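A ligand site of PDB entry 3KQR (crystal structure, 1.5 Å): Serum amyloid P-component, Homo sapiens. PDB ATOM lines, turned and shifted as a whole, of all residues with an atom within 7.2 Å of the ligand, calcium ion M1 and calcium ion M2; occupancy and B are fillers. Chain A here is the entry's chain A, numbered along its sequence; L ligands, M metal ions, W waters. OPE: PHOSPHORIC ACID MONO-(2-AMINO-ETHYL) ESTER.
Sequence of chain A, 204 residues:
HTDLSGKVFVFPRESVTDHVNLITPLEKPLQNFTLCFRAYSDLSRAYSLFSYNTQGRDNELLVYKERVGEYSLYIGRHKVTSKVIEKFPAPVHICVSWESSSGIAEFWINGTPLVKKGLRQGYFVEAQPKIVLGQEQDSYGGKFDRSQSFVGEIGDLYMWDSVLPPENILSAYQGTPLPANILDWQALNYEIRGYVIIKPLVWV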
ATOM      1  N   ALA A  46     -12.474  -9.145   2.104  1.00  0.00           N
ATOM      2  CA  ALA A  46     -12.906  -8.288   3.193  1.00  0.00           C
ATOM      3  C   ALA A  46     -14.024  -7.371   2.691  1.00  0.00           C
ATOM      4  O   ALA A  46     -14.078  -7.016   1.491  1.00  0.00           O
ATOM      5  CB  ALA A  46     -11.737  -7.446   3.699  1.00  0.00           C
ATOM      6  N   TYR A  47     -14.897  -6.961   3.602  1.00  0.00           N
ATOM      7  CA  TYR A  47     -15.923  -6.010   3.263  1.00  0.00           C
ATOM      8  C   TYR A  47     -16.459  -5.289   4.491  1.00  0.00           C
ATOM      9  O   TYR A  47     -16.400  -5.803   5.625  1.00  0.00           O
ATOM     10  CB  TYR A  47     -17.088  -6.662   2.512  1.00  0.00           C
ATOM     11  CG  TYR A  47     -17.686  -7.894   3.164  1.00  0.00           C
ATOM     12  CD1 TYR A  47     -18.694  -7.787   4.113  1.00  0.00           C
ATOM     13  CD2 TYR A  47     -17.283  -9.177   2.781  1.00  0.00           C
ATOM     14  CE1 TYR A  47     -19.285  -8.929   4.645  1.00  0.00           C
ATOM     15  CE2 TYR A  47     -17.827 -10.327   3.338  1.00  0.00           C
ATOM     16  CZ  TYR A  47     -18.840 -10.201   4.255  1.00  0.00           C
ATOM     17  OH  TYR A  47     -19.406 -11.366   4.738  1.00  0.00           O
ATOM     18  N   SER A  48     -16.983  -4.084   4.268  1.00  0.00           N
ATOM     19  CA  SER A  48     -17.644  -3.313   5.280  1.00  0.00           C
ATOM     20  C   SER A  48     -19.109  -3.737   5.463  1.00  0.00           C
ATOM     21  O   SER A  48     -19.840  -3.886   4.481  1.00  0.00           O
ATOM     22  CB  SER A  48     -17.611  -1.837   4.902  1.00  0.00           C
ATOM     23  OG  SER A  48     -18.305  -1.065   5.851  1.00  0.00           O
ATOM     24  N   SER A  51     -21.058   1.357   8.192  1.00  0.00           N
ATOM     25  CA  SER A  51     -20.096   2.450   8.142  1.00  0.00           C
ATOM     26  C   SER A  51     -20.739   3.727   8.675  1.00  0.00           C
ATOM     27  O   SER A  51     -21.749   4.211   8.131  1.00  0.00           O
ATOM     28  CB  SER A  51     -19.666   2.602   6.688  1.00  0.00           C
ATOM     29  OG  SER A  51     -18.822   3.717   6.452  1.00  0.00           O
ATOM     30  N   ASN A  53     -19.656   7.431   9.670  1.00  0.00           N
ATOM     31  CA  ASN A  53     -18.606   8.439   9.603  1.00  0.00           C
ATOM     32  C   ASN A  53     -19.209   9.750  10.084  1.00  0.00           C
ATOM     33  O   ASN A  53     -20.420   9.948  10.053  1.00  0.00           O
ATOM     34  CB  ASN A  53     -18.056   8.534   8.173  1.00  0.00           C
ATOM     35  CG  ASN A  53     -16.854   7.646   7.948  1.00  0.00           C
ATOM     36  OD1 ASN A  53     -16.567   6.735   8.744  1.00  0.00           O
ATOM     37  ND2 ASN A  53     -16.124   7.908   6.861  1.00  0.00           N
ATOM     38  N   ASP A  58     -13.118   9.667   9.817  1.00  0.00           N
ATOM     39  CA  ASP A  58     -13.281   8.373   9.133  1.00  0.00           C
ATOM     40  C   ASP A  58     -13.346   7.263  10.192  1.00  0.00           C
ATOM     41  O   ASP A  58     -12.724   7.364  11.265  1.00  0.00           O
ATOM     42  CB  ASP A  58     -12.088   8.087   8.194  1.00  0.00           C
ATOM     43  CG  ASP A  58     -12.318   6.887   7.257  1.00  0.00           C
ATOM     44  OD1 ASP A  58     -13.477   6.666   6.882  1.00  0.00           O
ATOM     45  OD2 ASP A  58     -11.350   6.178   6.882  1.00  0.00           O
ATOM     46  N   ASN A  59     -14.043   6.181   9.842  1.00  0.00           N
ATOM     47  CA  ASN A  59     -14.132   4.984  10.676  1.00  0.00           C
ATOM     48  C   ASN A  59     -14.563   5.332  12.088  1.00  0.00           C
ATOM     49  O   ASN A  59     -13.952   4.849  13.050  1.00  0.00           O
ATOM     50  CB  ASN A  59     -12.802   4.205  10.634  1.00  0.00           C
ATOM     51  CG  ASN A  59     -12.434   3.764   9.208  1.00  0.00           C
ATOM     52  OD1 ASN A  59     -13.241   3.910   8.288  1.00  0.00           O
ATOM     53  ND2 ASN A  59     -11.255   3.217   9.035  1.00  0.00           N
ATOM     54  N   GLU A  60     -15.556   6.222  12.227  1.00  0.00           N
ATOM     55  CA  GLU A  60     -15.925   6.663  13.578  1.00  0.00           C
ATOM     56  C   GLU A  60     -16.566   5.499  14.299  1.00  0.00           C
ATOM     57  O   GLU A  60     -16.277   5.252  15.471  1.00  0.00           O
ATOM     58  CB  GLU A  60     -16.792   7.935  13.621  1.00  0.00           C
ATOM     59  CG  GLU A  60     -17.200   8.401  15.006  1.00  0.00           C
ATOM     60  CD  GLU A  60     -16.059   8.999  15.820  1.00  0.00           C
ATOM     61  OE1 GLU A  60     -14.920   9.082  15.283  1.00  0.00           O
ATOM     62  OE2 GLU A  60     -16.350   9.394  16.949  1.00  0.00           O
ATOM     63  N   LEU A  62     -17.261   1.560  12.775  1.00  0.00           N
ATOM     64  CA  LEU A  62     -17.250   0.725  11.586  1.00  0.00           C
ATOM     65  C   LEU A  62     -17.258  -0.741  11.985  1.00  0.00           C
ATOM     66  O   LEU A  62     -16.430  -1.173  12.809  1.00  0.00           O
ATOM     67  CB  LEU A  62     -15.991   1.018  10.741  1.00  0.00           C
ATOM     68  CG  LEU A  62     -15.688   0.098   9.566  1.00  0.00           C
ATOM     69  CD1 LEU A  62     -16.748   0.140   8.472  1.00  0.00           C
ATOM     70  CD2 LEU A  62     -14.336   0.410   8.932  1.00  0.00           C
ATOM     71  N   TYR A  64     -16.637  -4.347  10.344  1.00  0.00           N
ATOM     72  CA  TYR A  64     -15.893  -4.765   9.162  1.00  0.00           C
ATOM     73  C   TYR A  64     -15.574  -6.246   9.251  1.00  0.00           C
ATOM     74  O   TYR A  64     -15.200  -6.736  10.295  1.00  0.00           O
ATOM     75  CB  TYR A  64     -14.567  -3.971   9.104  1.00  0.00           C
ATOM     76  CG  TYR A  64     -13.838  -4.018   7.770  1.00  0.00           C
ATOM     77  CD1 TYR A  64     -14.292  -3.250   6.700  1.00  0.00           C
ATOM     78  CD2 TYR A  64     -12.705  -4.784   7.589  1.00  0.00           C
ATOM     79  CE1 TYR A  64     -13.641  -3.256   5.497  1.00  0.00           C
ATOM     80  CE2 TYR A  64     -12.023  -4.777   6.364  1.00  0.00           C
ATOM     81  CZ  TYR A  64     -12.521  -4.010   5.341  1.00  0.00           C
ATOM     82  OH  TYR A  64     -11.889  -3.986   4.093  1.00  0.00           O
ATOM     83  N   GLU A  66     -13.091  -8.936   8.108  1.00  0.00           N
ATOM     84  CA  GLU A  66     -11.729  -9.071   7.594  1.00  0.00           C
ATOM     85  C   GLU A  66     -11.572 -10.278   6.647  1.00  0.00           C
ATOM     86  O   GLU A  66     -10.970 -10.220   5.555  1.00  0.00           O
ATOM     87  CB  GLU A  66     -10.805  -9.302   8.806  1.00  0.00           C
ATOM     88  CG  GLU A  66     -10.909  -8.269   9.943  1.00  0.00           C
ATOM     89  CD  GLU A  66     -10.306  -6.911   9.548  1.00  0.00           C
ATOM     90  OE1 GLU A  66      -9.724  -6.840   8.436  1.00  0.00           O
ATOM     91  OE2 GLU A  66     -10.413  -5.927  10.348  1.00  0.00           O
ATOM     92  N   SER A  72     -14.469  -7.285  13.034  1.00  0.00           N
ATOM     93  CA  SER A  72     -13.830  -6.128  13.631  1.00  0.00           C
ATOM     94  C   SER A  72     -14.785  -4.991  13.890  1.00  0.00           C
ATOM     95  O   SER A  72     -15.710  -4.741  13.117  1.00  0.00           O
ATOM     96  CB  SER A  72     -12.720  -5.604  12.731  1.00  0.00           C
ATOM     97  OG  SER A  72     -11.717  -6.605  12.543  1.00  0.00           O
ATOM     98  N   TYR A  74     -14.386  -0.867  14.663  1.00  0.00           N
ATOM     99  CA  TYR A  74     -13.609   0.346  14.839  1.00  0.00           C
ATOM    100  C   TYR A  74     -14.416   1.367  15.593  1.00  0.00           C
ATOM    101  O   TYR A  74     -15.609   1.566  15.317  1.00  0.00           O
ATOM    102  CB  TYR A  74     -13.248   0.952  13.490  1.00  0.00           C
ATOM    103  CG  TYR A  74     -12.306   0.157  12.637  1.00  0.00           C
ATOM    104  CD1 TYR A  74     -12.690  -1.001  12.031  1.00  0.00           C
ATOM    105  CD2 TYR A  74     -11.019   0.627  12.397  1.00  0.00           C
ATOM    106  CE1 TYR A  74     -11.817  -1.715  11.218  1.00  0.00           C
ATOM    107  CE2 TYR A  74     -10.150  -0.069  11.589  1.00  0.00           C
ATOM    108  CZ  TYR A  74     -10.542  -1.234  11.002  1.00  0.00           C
ATOM    109  OH  TYR A  74      -9.671  -1.925  10.181  1.00  0.00           O
ATOM    110  N   ARG A  77     -11.355   5.195  14.846  1.00  0.00           N
ATOM    111  CA  ARG A  77     -10.134   4.772  14.173  1.00  0.00           C
ATOM    112  C   ARG A  77      -9.321   3.683  14.876  1.00  0.00           C
ATOM    113  O   ARG A  77      -8.436   3.099  14.277  1.00  0.00           O
ATOM    114  CB  ARG A  77      -9.228   5.993  13.903  1.00  0.00           C
ATOM    115  CG  ARG A  77      -9.800   6.878  12.827  1.00  0.00           C
ATOM    116  CD  ARG A  77      -9.446   6.281  11.492  1.00  0.00           C
ATOM    117  NE  ARG A  77      -8.023   6.403  11.224  1.00  0.00           N
ATOM    118  CZ  ARG A  77      -7.503   7.308  10.406  1.00  0.00           C
ATOM    119  NH1 ARG A  77      -8.302   8.166   9.774  1.00  0.00           N
ATOM    120  NH2 ARG A  77      -6.192   7.351  10.227  1.00  0.00           N
ATOM    121  N   LYS A  79      -9.275  -0.146  16.598  1.00  0.00           N
ATOM    122  CA  LYS A  79     -10.028  -1.364  16.274  1.00  0.00           C
ATOM    123  C   LYS A  79      -9.762  -2.494  17.222  1.00  0.00           C
ATOM    124  O   LYS A  79      -8.706  -2.595  17.901  1.00  0.00           O
ATOM    125  CB  LYS A  79      -9.800  -1.830  14.839  1.00  0.00           C
ATOM    126  CG  LYS A  79      -8.428  -2.303  14.615  1.00  0.00           C
ATOM    127  CD  LYS A  79      -8.187  -2.684  13.156  1.00  0.00           C
ATOM    128  CE  LYS A  79      -8.906  -3.963  12.809  1.00  0.00           C
ATOM    129  NZ  LYS A  79      -8.352  -4.519  11.539  1.00  0.00           N
ATOM    130  N   GLU A 136     -18.001   1.191   2.184  1.00  0.00           N
ATOM    131  CA  GLU A 136     -17.202   1.732   3.246  1.00  0.00           C
ATOM    132  C   GLU A 136     -16.860   3.197   2.930  1.00  0.00           C
ATOM    133  O   GLU A 136     -16.333   3.486   1.866  1.00  0.00           O
ATOM    134  CB  GLU A 136     -15.929   0.878   3.352  1.00  0.00           C
ATOM    135  CG  GLU A 136     -15.354   0.842   4.713  1.00  0.00           C
ATOM    136  CD  GLU A 136     -14.563   2.076   5.009  1.00  0.00           C
ATOM    137  OE1 GLU A 136     -13.756   2.483   4.126  1.00  0.00           O
ATOM    138  OE2 GLU A 136     -14.701   2.634   6.118  1.00  0.00           O
ATOM    139  N   GLN A 137     -17.197   4.105   3.836  1.00  0.00           N
ATOM    140  CA  GLN A 137     -16.941   5.517   3.605  1.00  0.00           C
ATOM    141  C   GLN A 137     -15.510   5.829   3.920  1.00  0.00           C
ATOM    142  O   GLN A 137     -14.988   5.358   4.928  1.00  0.00           O
ATOM    143  CB  GLN A 137     -17.813   6.390   4.491  1.00  0.00           C
ATOM    144  CG  GLN A 137     -19.299   6.279   4.248  1.00  0.00           C
ATOM    145  CD  GLN A 137     -20.066   7.038   5.304  1.00  0.00           C
ATOM    146  OE1 GLN A 137     -20.250   8.249   5.212  1.00  0.00           O
ATOM    147  NE2 GLN A 137     -20.479   6.328   6.359  1.00  0.00           N
ATOM    148  N   ASP A 138     -14.884   6.647   3.110  1.00  0.00           N
ATOM    149  CA  ASP A 138     -13.609   7.246   3.499  1.00  0.00           C
ATOM    150  C   ASP A 138     -13.780   8.764   3.670  1.00  0.00           C
ATOM    151  O   ASP A 138     -12.864   9.452   4.135  1.00  0.00           O
ATOM    152  CB  ASP A 138     -12.501   6.907   2.503  1.00  0.00           C
ATOM    153  CG  ASP A 138     -11.939   5.514   2.708  1.00  0.00           C
ATOM    154  OD1 ASP A 138     -12.196   4.930   3.799  1.00  0.00           O
ATOM    155  OD2 ASP A 138     -11.230   4.970   1.818  1.00  0.00           O
ATOM    156  N   SER A 139     -14.975   9.277   3.338  1.00  0.00           N
ATOM    157  CA  SER A 139     -15.316  10.685   3.589  1.00  0.00           C
ATOM    158  C   SER A 139     -16.653  10.788   4.334  1.00  0.00           C
ATOM    159  O   SER A 139     -17.242   9.773   4.690  1.00  0.00           O
ATOM    160  CB  SER A 139     -15.408  11.428   2.269  1.00  0.00           C
ATOM    161  OG  SER A 139     -16.606  11.064   1.598  1.00  0.00           O
ATOM    162  N   GLY A 142     -19.126   9.514   1.488  1.00  0.00           N
ATOM    163  CA  GLY A 142     -18.620   9.057   0.207  1.00  0.00           C
ATOM    164  C   GLY A 142     -17.221   8.475   0.228  1.00  0.00           C
ATOM    165  O   GLY A 142     -16.804   7.863   1.208  1.00  0.00           O
ATOM    166  N   LYS A 143     -16.497   8.655  -0.878  1.00  0.00           N
ATOM    167  CA  LYS A 143     -15.163   8.085  -1.048  1.00  0.00           C
ATOM    168  C   LYS A 143     -15.177   6.578  -0.841  1.00  0.00           C
ATOM    169  O   LYS A 143     -14.426   6.038  -0.024  1.00  0.00           O
ATOM    170  CB  LYS A 143     -14.153   8.715  -0.075  1.00  0.00           C
ATOM    171  CG  LYS A 143     -13.647  10.100  -0.480  1.00  0.00           C
ATOM    172  CD  LYS A 143     -12.326  10.004  -1.225  1.00  0.00           C
ATOM    173  CE  LYS A 143     -11.653  11.368  -1.342  1.00  0.00           C
ATOM    174  NZ  LYS A 143     -11.174  11.877  -0.020  1.00  0.00           N
ATOM    175  N   PHE A 144     -16.052   5.905  -1.581  1.00  0.00           N
ATOM    176  CA  PHE A 144     -16.166   4.458  -1.531  1.00  0.00           C
ATOM    177  C   PHE A 144     -15.018   3.734  -2.241  1.00  0.00           C
ATOM    178  O   PHE A 144     -14.246   4.316  -2.983  1.00  0.00           O
ATOM    179  CB  PHE A 144     -17.517   4.049  -2.114  1.00  0.00           C
ATOM    180  CG  PHE A 144     -18.701   4.783  -1.502  1.00  0.00           C
ATOM    181  CD1 PHE A 144     -18.737   5.064  -0.141  1.00  0.00           C
ATOM    182  CD2 PHE A 144     -19.775   5.165  -2.281  1.00  0.00           C
ATOM    183  CE1 PHE A 144     -19.836   5.710   0.430  1.00  0.00           C
ATOM    184  CE2 PHE A 144     -20.871   5.820  -1.736  1.00  0.00           C
ATOM    185  CZ  PHE A 144     -20.907   6.100  -0.375  1.00  0.00           C
ATOM    186  N   ASP A 145     -14.919   2.439  -1.992  1.00  0.00           N
ATOM    187  CA  ASP A 145     -13.869   1.593  -2.528  1.00  0.00           C
ATOM    188  C   ASP A 145     -14.502   0.267  -2.910  1.00  0.00           C
ATOM    189  O   ASP A 145     -15.014  -0.448  -2.046  1.00  0.00           O
ATOM    190  CB  ASP A 145     -12.796   1.389  -1.454  1.00  0.00           C
ATOM    191  CG  ASP A 145     -11.691   0.419  -1.859  1.00  0.00           C
ATOM    192  OD1 ASP A 145     -11.834  -0.310  -2.861  1.00  0.00           O
ATOM    193  OD2 ASP A 145     -10.651   0.389  -1.145  1.00  0.00           O
ATOM    194  N   GLN A 148     -14.044  -2.952  -0.938  1.00  0.00           N
ATOM    195  CA  GLN A 148     -14.640  -3.083   0.407  1.00  0.00           C
ATOM    196  C   GLN A 148     -16.164  -3.101   0.361  1.00  0.00           C
ATOM    197  O   GLN A 148     -16.830  -3.115   1.407  1.00  0.00           O
ATOM    198  CB  GLN A 148     -14.223  -1.931   1.306  1.00  0.00           C
ATOM    199  CG  GLN A 148     -12.735  -1.774   1.362  1.00  0.00           C
ATOM    200  CD  GLN A 148     -12.352  -0.634   2.208  1.00  0.00           C
ATOM    201  OE1 GLN A 148     -12.704   0.507   1.918  1.00  0.00           O
ATOM    202  NE2 GLN A 148     -11.649  -0.921   3.318  1.00  0.00           N
HETATM  203  CA  OPE L   1     -11.201   0.219   7.082  1.00  0.00           C
HETATM  204  CB  OPE L   1     -11.199  -1.277   7.264  1.00  0.00           C
HETATM  205  O1  OPE L   1     -10.292   1.996   3.780  1.00  0.00           O
HETATM  206  O2  OPE L   1      -8.797   2.144   5.812  1.00  0.00           O
HETATM  207  O3  OPE L   1     -11.164   2.989   5.988  1.00  0.00           O
HETATM  208  O4  OPE L   1     -10.704   0.423   5.786  1.00  0.00           O
HETATM  209  N   OPE L   1      -9.806  -1.753   7.138  1.00  0.00           N
HETATM  210  P   OPE L   1     -10.337   1.947   5.356  1.00  0.00           P
HETATM  211 CA    CA M   1     -12.078   2.707   2.495  1.00  0.00          CA
HETATM  212 CA    CA M   2     -13.062   4.358   5.921  1.00  0.00          CA
HETATM  213  O   HOH W   1      -8.827  -4.354   7.791  1.00  0.00           O
HETATM  214  O   HOH W   2     -13.837   3.467   0.952  1.00  0.00           O
HETATM  215  O   HOH W   3      -8.842  -2.086   4.695  1.00  0.00           O
HETATM  216  O   HOH W   4      -8.651   4.882   6.586  1.00  0.00           O
HETATM  217  O   HOH W   5      -8.562   0.121   2.794  1.00  0.00           O
HETATM  218  O   HOH W   6     -10.471   2.276   0.774  1.00  0.00           O
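Merely in contact with the ligand: Tyr 64 and Leu 62.
Hydrophobic or aromatic side chains that line the ligand: Leu 62, Tyr 64 and Tyr 74.
Of the 24 residues printed, 8 come within 4 Å of the ligand.
Along chain A the residues within 4 Å of the ligand span positions 58 to 148.
Calcium ion M2 is bound by O3 of the ligand (2.3 Å), OD1 of Asp 138 (2.4 Å), OE2 of Glu 136 (2.4 Å), O of Gln 137 (2.4 Å), OD1 of Asn 59 (2.4 Å), OD1 of Asp 58 (2.5 Å), OD2 of Asp 58 (2.7 Å) and OE1 of Glu 136 (2.7 Å).
An oxygen (O1) of the ligand binds calcium ion M1 (2.3 Å).
OE1 of Glu 136 is bound to calcium ion M1, at 2.4 Å.
Calcium ion M1 is bound by the side-chain amide oxygen (OE1) of Gln 148, 2.4 Å away.
Water W6 binds calcium ion M1 (2.4 Å).
Water W2 is bound to calcium ion M1 (2.5 Å).
Calcium ion M1 is bound by the side-chain carboxylate (OD2) of Asp 138 (2.5 Å).
OD1 of Asp 138 binds calcium ion M1 (2.6 Å).
OH of Tyr 74 lies within hydrogen-bond range of N of the ligand, 3.1 Å away.
Five residues have an atom within 4 Å of calcium ion M2: Asp 58, Asn 59, Glu 136, Gln 137 and Asp 138.
Along chain A the residues within 4 Å of calcium ion M2 span positions 58 to 138.
Water W2 lies within hydrogen-bond range of the backbone carbonyl oxygen (O) of Glu 136, the backbone carbonyl oxygen (O) of Lys 143 and the backbone NH (N) of Asp 145.
Water W3 lies within hydrogen-bond range of a nitrogen (N) of the ligand (2.6 Å) and the side-chain amide nitrogen of Gln 148 (3.3 Å).
Water W1 bridges the side-chain carboxylate of Glu 66 (2.7 Å) and a nitrogen (N) of the ligand (2.9 Å).
NE2 of Gln 148 is in hydrogen-bond range of OH of Tyr 64, at 3.2 Å.
OD1 of Asn 53 is in hydrogen-bond range of N of Asn 59, at 2.8 Å.
The backbone NH (N) of Ser 48 sits at hydrogen-bond distance from the backbone carbonyl oxygen (O) of Gln 148, 3.0 Å away.
The backbone carbonyl oxygen (O) of Ser 139 lies close to the side-chain amide oxygen (OE1) of Gln 137 (3.4 Å).
The side-chain hydroxyl (OH) of Tyr 74 sits at hydrogen-bond distance from the side-chain amino group (NZ) of Lys 79 (3.2 Å).
N of Ser 72 lies within hydrogen-bond range of O of Tyr 64 (2.9 Å).
The backbone carbonyl oxygen (O) of Asn 59 sits at hydrogen-bond distance from the backbone NH (N) of Arg 77 (3.2 Å).
N of Asp 138 sits at hydrogen-bond distance from O of Lys 143 (3.2 Å).
The nearest printed residue that does not touch calcium ion M1 is Asp 145 (4.2 Å).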
